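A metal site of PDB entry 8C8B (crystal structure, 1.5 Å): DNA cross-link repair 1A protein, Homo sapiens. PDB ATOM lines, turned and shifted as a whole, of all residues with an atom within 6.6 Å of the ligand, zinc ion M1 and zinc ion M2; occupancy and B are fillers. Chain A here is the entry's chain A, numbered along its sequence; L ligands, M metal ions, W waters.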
ATOM      1  N   HIS A  35     -24.549  13.635  27.014  1.00  0.00           N
ATOM      2  CA  HIS A  35     -23.524  13.656  28.044  1.00  0.00           C
ATOM      3  C   HIS A  35     -22.141  13.705  27.401  1.00  0.00           C
ATOM      4  O   HIS A  35     -21.988  13.438  26.206  1.00  0.00           O
ATOM      5  CB  HIS A  35     -23.639  12.464  29.001  1.00  0.00           C
ATOM      6  CG  HIS A  35     -23.370  11.125  28.382  1.00  0.00           C
ATOM      7  ND1 HIS A  35     -24.188  10.560  27.426  1.00  0.00           N
ATOM      8  CD2 HIS A  35     -22.410  10.214  28.633  1.00  0.00           C
ATOM      9  CE1 HIS A  35     -23.729   9.370  27.108  1.00  0.00           C
ATOM     10  NE2 HIS A  35     -22.644   9.141  27.815  1.00  0.00           N
ATOM     11  N   PHE A  36     -21.140  14.037  28.226  1.00  0.00           N
ATOM     12  CA  PHE A  36     -19.783  14.302  27.749  1.00  0.00           C
ATOM     13  C   PHE A  36     -18.933  13.027  27.811  1.00  0.00           C
ATOM     14  O   PHE A  36     -18.004  12.876  28.620  1.00  0.00           O
ATOM     15  CB  PHE A  36     -19.156  15.444  28.552  1.00  0.00           C
ATOM     16  CG  PHE A  36     -17.876  15.990  27.962  1.00  0.00           C
ATOM     17  CD1 PHE A  36     -17.910  16.842  26.869  1.00  0.00           C
ATOM     18  CD2 PHE A  36     -16.647  15.657  28.504  1.00  0.00           C
ATOM     19  CE1 PHE A  36     -16.740  17.353  26.330  1.00  0.00           C
ATOM     20  CE2 PHE A  36     -15.469  16.145  27.969  1.00  0.00           C
ATOM     21  CZ  PHE A  36     -15.514  17.006  26.877  1.00  0.00           C
ATOM     22  N   HIS A  37     -19.295  12.072  26.953  1.00  0.00           N
ATOM     23  CA  HIS A  37     -18.484  10.882  26.712  1.00  0.00           C
ATOM     24  C   HIS A  37     -18.136  10.841  25.234  1.00  0.00           C
ATOM     25  O   HIS A  37     -18.981  11.137  24.373  1.00  0.00           O
ATOM     26  CB  HIS A  37     -19.216   9.610  27.127  1.00  0.00           C
ATOM     27  CG  HIS A  37     -19.084   9.295  28.588  1.00  0.00           C
ATOM     28  ND1 HIS A  37     -19.935   8.432  29.239  1.00  0.00           N
ATOM     29  CD2 HIS A  37     -18.202   9.723  29.520  1.00  0.00           C
ATOM     30  CE1 HIS A  37     -19.585   8.324  30.508  1.00  0.00           C
ATOM     31  NE2 HIS A  37     -18.532   9.101  30.704  1.00  0.00           N
ATOM     32  N   SER A  38     -16.881  10.475  24.940  1.00  0.00           N
ATOM     33  CA  SER A  38     -16.326  10.677  23.603  1.00  0.00           C
ATOM     34  C   SER A  38     -17.132   9.983  22.513  1.00  0.00           C
ATOM     35  O   SER A  38     -17.247  10.511  21.408  1.00  0.00           O
ATOM     36  CB  SER A  38     -14.858  10.259  23.557  1.00  0.00           C
ATOM     37  OG  SER A  38     -14.702   8.875  23.796  1.00  0.00           O
ATOM     38  N   ASP A  39     -17.691   8.804  22.805  1.00  0.00           N
ATOM     39  CA  ASP A  39     -18.515   8.132  21.798  1.00  0.00           C
ATOM     40  C   ASP A  39     -19.795   8.889  21.469  1.00  0.00           C
ATOM     41  O   ASP A  39     -20.472   8.546  20.494  1.00  0.00           O
ATOM     42  CB  ASP A  39     -18.804   6.670  22.163  1.00  0.00           C
ATOM     43  CG  ASP A  39     -19.225   6.495  23.614  1.00  0.00           C
ATOM     44  OD1 ASP A  39     -18.617   7.134  24.501  1.00  0.00           O
ATOM     45  OD2 ASP A  39     -20.159   5.700  23.870  1.00  0.00           O
ATOM     46  N   HIS A  40     -20.135   9.924  22.232  1.00  0.00           N
ATOM     47  CA  HIS A  40     -21.322  10.743  21.972  1.00  0.00           C
ATOM     48  C   HIS A  40     -21.015  12.130  21.455  1.00  0.00           C
ATOM     49  O   HIS A  40     -21.764  12.637  20.613  1.00  0.00           O
ATOM     50  CB  HIS A  40     -22.179  10.852  23.240  1.00  0.00           C
ATOM     51  CG  HIS A  40     -22.601   9.528  23.763  1.00  0.00           C
ATOM     52  ND1 HIS A  40     -23.907   9.080  23.685  1.00  0.00           N
ATOM     53  CD2 HIS A  40     -21.889   8.522  24.305  1.00  0.00           C
ATOM     54  CE1 HIS A  40     -23.972   7.859  24.191  1.00  0.00           C
ATOM     55  NE2 HIS A  40     -22.764   7.504  24.569  1.00  0.00           N
ATOM     56  N   HIS A  96     -26.165   8.432  35.041  1.00  0.00           N
ATOM     57  CA  HIS A  96     -25.031   7.875  34.304  1.00  0.00           C
ATOM     58  C   HIS A  96     -23.786   8.550  34.858  1.00  0.00           C
ATOM     59  O   HIS A  96     -23.396   8.272  35.994  1.00  0.00           O
ATOM     60  CB  HIS A  96     -25.288   8.067  32.804  1.00  0.00           C
ATOM     61  CG  HIS A  96     -24.241   7.478  31.911  1.00  0.00           C
ATOM     62  ND1 HIS A  96     -23.856   6.155  31.952  1.00  0.00           N
ATOM     63  CD2 HIS A  96     -23.498   8.053  30.935  1.00  0.00           C
ATOM     64  CE1 HIS A  96     -22.925   5.939  31.049  1.00  0.00           C
ATOM     65  NE2 HIS A  96     -22.686   7.083  30.429  1.00  0.00           N
ATOM     66  N   CYS A  97     -23.188   9.473  34.126  1.00  0.00           N
ATOM     67  CA  CYS A  97     -22.060  10.260  34.610  1.00  0.00           C
ATOM     68  C   CYS A  97     -22.517  11.693  34.891  1.00  0.00           C
ATOM     69  O   CYS A  97     -23.661  12.062  34.606  1.00  0.00           O
ATOM     70  CB  CYS A  97     -20.952  10.254  33.550  1.00  0.00           C
ATOM     71  SG  CYS A  97     -21.422  11.106  32.028  1.00  0.00           S
ATOM     72  N   ASP A 118     -27.273   7.549  27.543  1.00  0.00           N
ATOM     73  CA  ASP A 118     -26.831   6.461  28.408  1.00  0.00           C
ATOM     74  C   ASP A 118     -27.436   6.655  29.787  1.00  0.00           C
ATOM     75  O   ASP A 118     -27.468   7.771  30.309  1.00  0.00           O
ATOM     76  CB  ASP A 118     -25.307   6.442  28.547  1.00  0.00           C
ATOM     77  CG  ASP A 118     -24.601   5.934  27.326  1.00  0.00           C
ATOM     78  OD1 ASP A 118     -25.293   5.438  26.406  1.00  0.00           O
ATOM     79  OD2 ASP A 118     -23.353   6.033  27.301  1.00  0.00           O
ATOM     80  N   ASP A 141     -31.072   2.908  25.935  1.00  0.00           N
ATOM     81  CA  ASP A 141     -29.706   2.433  26.153  1.00  0.00           C
ATOM     82  C   ASP A 141     -29.786   0.961  26.506  1.00  0.00           C
ATOM     83  O   ASP A 141     -30.112   0.596  27.649  1.00  0.00           O
ATOM     84  CB  ASP A 141     -29.054   3.252  27.260  1.00  0.00           C
ATOM     85  CG  ASP A 141     -27.734   2.665  27.756  1.00  0.00           C
ATOM     86  OD1 ASP A 141     -27.167   1.786  27.081  1.00  0.00           O
ATOM     87  OD2 ASP A 141     -27.290   3.071  28.847  1.00  0.00           O
ATOM     88  N   THR A 143     -27.259  -1.250  26.492  1.00  0.00           N
ATOM     89  CA  THR A 143     -25.896  -1.761  26.645  1.00  0.00           C
ATOM     90  C   THR A 143     -25.888  -3.175  27.210  1.00  0.00           C
ATOM     91  O   THR A 143     -25.216  -4.065  26.683  1.00  0.00           O
ATOM     92  CB  THR A 143     -25.064  -0.816  27.528  1.00  0.00           C
ATOM     93  OG1 THR A 143     -24.931   0.449  26.868  1.00  0.00           O
ATOM     94  CG2 THR A 143     -23.670  -1.381  27.779  1.00  0.00           C
ATOM     95  N   TYR A 144     -26.637  -3.408  28.284  1.00  0.00           N
ATOM     96  CA  TYR A 144     -26.628  -4.682  29.000  1.00  0.00           C
ATOM     97  C   TYR A 144     -27.983  -5.381  28.941  1.00  0.00           C
ATOM     98  O   TYR A 144     -28.474  -5.941  29.927  1.00  0.00           O
ATOM     99  CB  TYR A 144     -26.192  -4.486  30.452  1.00  0.00           C
ATOM    100  CG  TYR A 144     -24.747  -4.072  30.596  1.00  0.00           C
ATOM    101  CD1 TYR A 144     -23.735  -4.779  29.966  1.00  0.00           C
ATOM    102  CD2 TYR A 144     -24.392  -2.963  31.370  1.00  0.00           C
ATOM    103  CE1 TYR A 144     -22.406  -4.410  30.109  1.00  0.00           C
ATOM    104  CE2 TYR A 144     -23.079  -2.589  31.498  1.00  0.00           C
ATOM    105  CZ  TYR A 144     -22.092  -3.314  30.870  1.00  0.00           C
ATOM    106  OH  TYR A 144     -20.779  -2.933  31.021  1.00  0.00           O
ATOM    107  N   TYR A 182     -10.614   7.020  32.782  1.00  0.00           N
ATOM    108  CA  TYR A 182     -10.399   7.425  31.395  1.00  0.00           C
ATOM    109  C   TYR A 182     -11.401   8.446  30.868  1.00  0.00           C
ATOM    110  O   TYR A 182     -11.202   8.972  29.772  1.00  0.00           O
ATOM    111  CB  TYR A 182     -10.335   6.225  30.431  1.00  0.00           C
ATOM    112  CG  TYR A 182     -11.446   5.207  30.573  1.00  0.00           C
ATOM    113  CD1 TYR A 182     -12.789   5.572  30.486  1.00  0.00           C
ATOM    114  CD2 TYR A 182     -11.156   3.856  30.740  1.00  0.00           C
ATOM    115  CE1 TYR A 182     -13.796   4.633  30.592  1.00  0.00           C
ATOM    116  CE2 TYR A 182     -12.158   2.911  30.853  1.00  0.00           C
ATOM    117  CZ  TYR A 182     -13.469   3.298  30.779  1.00  0.00           C
ATOM    118  OH  TYR A 182     -14.469   2.366  30.887  1.00  0.00           O
ATOM    119  N   SER A 183     -12.470   8.733  31.611  1.00  0.00           N
ATOM    120  CA  SER A 183     -13.481   9.705  31.203  1.00  0.00           C
ATOM    121  C   SER A 183     -14.146  10.188  32.479  1.00  0.00           C
ATOM    122  O   SER A 183     -13.809   9.747  33.579  1.00  0.00           O
ATOM    123  CB  SER A 183     -14.498   9.040  30.274  1.00  0.00           C
ATOM    124  OG  SER A 183     -15.047   7.881  30.881  1.00  0.00           O
ATOM    125  N   ILE A 184     -15.108  11.103  32.330  1.00  0.00           N
ATOM    126  CA  ILE A 184     -15.917  11.431  33.487  1.00  0.00           C
ATOM    127  C   ILE A 184     -16.827  10.258  33.832  1.00  0.00           C
ATOM    128  O   ILE A 184     -17.035   9.338  33.033  1.00  0.00           O
ATOM    129  CB  ILE A 184     -16.731  12.723  33.285  1.00  0.00           C
ATOM    130  CG1 ILE A 184     -17.757  12.544  32.165  1.00  0.00           C
ATOM    131  CG2 ILE A 184     -15.812  13.904  33.036  1.00  0.00           C
ATOM    132  CD1 ILE A 184     -18.782  13.674  32.114  1.00  0.00           C
ATOM    133  N   LYS A 186     -18.028   7.755  37.504  1.00  0.00           N
ATOM    134  CA  LYS A 186     -17.436   6.869  38.499  1.00  0.00           C
ATOM    135  C   LYS A 186     -16.553   7.598  39.499  1.00  0.00           C
ATOM    136  O   LYS A 186     -15.738   6.976  40.177  1.00  0.00           O
ATOM    137  CB  LYS A 186     -16.717   5.677  37.848  1.00  0.00           C
ATOM    138  CG  LYS A 186     -17.546   5.026  36.722  1.00  0.00           C
ATOM    139  CD  LYS A 186     -16.928   3.748  36.177  1.00  0.00           C
ATOM    140  CE  LYS A 186     -17.759   3.209  35.002  1.00  0.00           C
ATOM    141  NZ  LYS A 186     -17.357   1.826  34.619  1.00  0.00           N
ATOM    142  N   GLY A 266     -16.872  -2.187  33.748  1.00  0.00           N
ATOM    143  CA  GLY A 266     -18.302  -2.385  33.628  1.00  0.00           C
ATOM    144  C   GLY A 266     -18.665  -3.756  34.123  1.00  0.00           C
ATOM    145  O   GLY A 266     -18.204  -4.179  35.190  1.00  0.00           O
ATOM    146  N   TRP A 267     -19.491  -4.478  33.373  1.00  0.00           N
ATOM    147  CA  TRP A 267     -19.798  -5.859  33.703  1.00  0.00           C
ATOM    148  C   TRP A 267     -18.658  -6.760  33.264  1.00  0.00           C
ATOM    149  O   TRP A 267     -18.042  -6.552  32.221  1.00  0.00           O
ATOM    150  CB  TRP A 267     -21.077  -6.295  32.993  1.00  0.00           C
ATOM    151  CG  TRP A 267     -21.295  -7.784  32.988  1.00  0.00           C
ATOM    152  CD1 TRP A 267     -21.964  -8.526  33.919  1.00  0.00           C
ATOM    153  CD2 TRP A 267     -20.835  -8.718  31.992  1.00  0.00           C
ATOM    154  NE1 TRP A 267     -21.953  -9.861  33.568  1.00  0.00           N
ATOM    155  CE2 TRP A 267     -21.266 -10.001  32.385  1.00  0.00           C
ATOM    156  CE3 TRP A 267     -20.096  -8.587  30.809  1.00  0.00           C
ATOM    157  CZ2 TRP A 267     -20.980 -11.143  31.641  1.00  0.00           C
ATOM    158  CZ3 TRP A 267     -19.821  -9.719  30.066  1.00  0.00           C
ATOM    159  CH2 TRP A 267     -20.261 -10.985  30.484  1.00  0.00           C
ATOM    160  N   GLU A 296     -22.241   2.375  35.354  1.00  0.00           N
ATOM    161  CA  GLU A 296     -23.152   3.498  35.128  1.00  0.00           C
ATOM    162  C   GLU A 296     -24.167   3.224  34.018  1.00  0.00           C
ATOM    163  O   GLU A 296     -24.778   4.158  33.502  1.00  0.00           O
ATOM    164  CB  GLU A 296     -22.374   4.820  34.950  1.00  0.00           C
ATOM    165  CG  GLU A 296     -21.798   5.283  36.312  1.00  0.00           C
ATOM    166  CD  GLU A 296     -20.999   6.576  36.281  1.00  0.00           C
ATOM    167  OE1 GLU A 296     -20.594   7.033  35.197  1.00  0.00           O
ATOM    168  OE2 GLU A 296     -20.780   7.144  37.385  1.00  0.00           O
ATOM    169  N   HIS A 297     -24.370   1.946  33.681  1.00  0.00           N
ATOM    170  CA  HIS A 297     -25.445   1.519  32.789  1.00  0.00           C
ATOM    171  C   HIS A 297     -26.368   0.572  33.542  1.00  0.00           C
ATOM    172  O   HIS A 297     -25.925  -0.129  34.464  1.00  0.00           O
ATOM    173  CB  HIS A 297     -24.916   0.761  31.558  1.00  0.00           C
ATOM    174  CG  HIS A 297     -24.100   1.606  30.613  1.00  0.00           C
ATOM    175  ND1 HIS A 297     -24.669   2.397  29.636  1.00  0.00           N
ATOM    176  CD2 HIS A 297     -22.760   1.768  30.496  1.00  0.00           C
ATOM    177  CE1 HIS A 297     -23.715   3.015  28.970  1.00  0.00           C
ATOM    178  NE2 HIS A 297     -22.547   2.652  29.467  1.00  0.00           N
ATOM    179  N   VAL A 319     -27.957   0.777  21.417  1.00  0.00           N
ATOM    180  CA  VAL A 319     -26.703   0.065  21.667  1.00  0.00           C
ATOM    181  C   VAL A 319     -26.880  -1.385  21.253  1.00  0.00           C
ATOM    182  O   VAL A 319     -27.974  -1.952  21.358  1.00  0.00           O
ATOM    183  CB  VAL A 319     -26.234   0.168  23.146  1.00  0.00           C
ATOM    184  CG1 VAL A 319     -24.833  -0.438  23.368  1.00  0.00           C
ATOM    185  CG2 VAL A 319     -26.221   1.622  23.595  1.00  0.00           C
HETATM  186  C1  LIG L   1     -17.372   5.826  29.660  1.00  0.00           C
HETATM  187  C2  LIG L   1     -16.832   3.381  24.088  1.00  0.00           C
HETATM  188  C3  LIG L   1     -18.312   2.339  25.549  1.00  0.00           C
HETATM  189  C4  LIG L   1     -19.221   1.199  25.815  1.00  0.00           C
HETATM  190  C5  LIG L   1     -19.833   0.180  27.951  1.00  0.00           C
HETATM  191  C6  LIG L   1     -19.962  -1.191  27.433  1.00  0.00           C
HETATM  192  C7  LIG L   1     -19.056  -2.122  27.467  1.00  0.00           C
HETATM  193  C8  LIG L   1     -17.989   5.123  28.463  1.00  0.00           C
HETATM  194  C9  LIG L   1     -19.401   5.636  28.207  1.00  0.00           C
HETATM  195  C10 LIG L   1     -17.313   4.292  26.278  1.00  0.00           C
HETATM  196  C11 LIG L   1     -16.597   4.406  25.033  1.00  0.00           C
HETATM  197  C12 LIG L   1     -15.710   5.455  24.712  1.00  0.00           C
HETATM  198  C13 LIG L   1     -15.088   5.480  23.501  1.00  0.00           C
HETATM  199  C14 LIG L   1     -15.328   4.459  22.564  1.00  0.00           C
HETATM  200  C15 LIG L   1     -16.171   3.434  22.842  1.00  0.00           C
HETATM  201  N1  LIG L   1     -19.610   6.298  27.080  1.00  0.00           N
HETATM  202  N2  LIG L   1     -17.147   5.236  27.246  1.00  0.00           N
HETATM  203  N3  LIG L   1     -17.693   2.348  24.357  1.00  0.00           N
HETATM  204  N4  LIG L   1     -19.927   1.229  26.953  1.00  0.00           N
HETATM  205  N5  LIG L   1     -18.137   3.263  26.507  1.00  0.00           N
HETATM  206  O1  LIG L   1     -20.885   6.779  26.781  1.00  0.00           O
HETATM  207  O2  LIG L   1     -20.292   5.420  29.023  1.00  0.00           O
HETATM  208  O3  LIG L   1     -19.248   0.246  25.034  1.00  0.00           O
HETATM  209 ZN    ZN M   1     -21.671   7.278  28.487  1.00  0.00          ZN
HETATM  210 ZN    ZN M   2     -22.085   5.671  25.643  1.00  0.00          ZN
HETATM  211  O   HOH W   1     -23.504   4.397  24.862  1.00  0.00           O
HETATM  212  O   HOH W   2     -22.812   1.727  25.477  1.00  0.00           O
HETATM  213  O   HOH W   3     -21.295   3.864  26.814  1.00  0.00           O
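The side-chain carboxylate (OD1) of Asp 39 sits at hydrogen-bond distance from a nitrogen (N1) of the ligand.
The backbone carbonyl oxygen of Glu 296 is in hydrogen-bond range of a ring nitrogen (ND1) of His 96.
A ring nitrogen (NE2) of His 37 sits at hydrogen-bond distance from the backbone carbonyl oxygen of Ile 184 (2.8 Å).
NE2 of His 37 lies close to SG of Cys 97.
NE2 of His 40 lies close to OD2 of Asp 39, at 3.2 Å.
ND1 of His 297 lies within hydrogen-bond range of OG1 of Thr 143 (3.4 Å).
A ring nitrogen (ND1) of His 297 sits at hydrogen-bond distance from the side-chain carboxylate (OD2) of Asp 141 (2.8 Å).
OG1 of Thr 143 is in hydrogen-bond range of OD1 of Asp 141 (2.6 Å).
Ser 38 touches the ligand (OG to C13, 3.4 Å).
Thr 143 touches the ligand.
Tyr 182 touches the ligand (CE1 to C1, 3.9 Å).
OG of Ser 183 touches C1 of the ligand (3.3 Å).
His 297 touches the ligand.
Hydrophobic or aromatic side chains within 4 Å of the ligand: His 35, His 37, His 40, His 96 and Tyr 182.
Within 4 Å of the ligand: His 35, His 37, Ser 38, Asp 39, His 40, His 96, Asp 118, Thr 143, Tyr 182, Ser 183 and His 297.
Along chain A the residues within 4 Å of the ligand span positions 35 to 297.
The nearest printed residue that does not touch the ligand is Tyr 144 (4.03 Å).
Four residues have an atom within 4 Å of zinc ion M1: His 35, His 37, His 96 and Asp 118.
The nearest printed residue that does not touch zinc ion M2 is His 35 (4.1 Å).
Zinc ion M1 is bound by O1 of the ligand (1.9 Å).
A ring nitrogen (NE2) of His 96 is bound to zinc ion M1 (2.2 Å).
Zinc ion M1 is bound by NE2 of His 35, 2.2 Å away.
Zinc ion M1 is bound by ND1 of His 37 (2.2 Å).
Zinc ion M1 is bound by an oxygen (O2) of the ligand.
Zinc ion M1 is bound by OD2 of Asp 118 (2.4 Å).
Zinc ion M1 has six donor atoms within binding distance.
Zinc ion M2 is bound by O1 of the ligand (2.0 Å), water W1 (2.1 Å), OD2 of Asp 118 (2.1 Å), NE2 of His 40 (2.2 Å) and water W3 (2.3 Å).
Zinc ion M2 has five donor atoms within binding distance.
Slightly farther from zinc ion M2 lies OD2 of Asp 39 (2.6 Å).
Water W3 bridges N4 of the ligand and NE2 of His 297.
Water W2 lies within hydrogen-bond range of OG1 of Thr 143 and N4 of the ligand.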
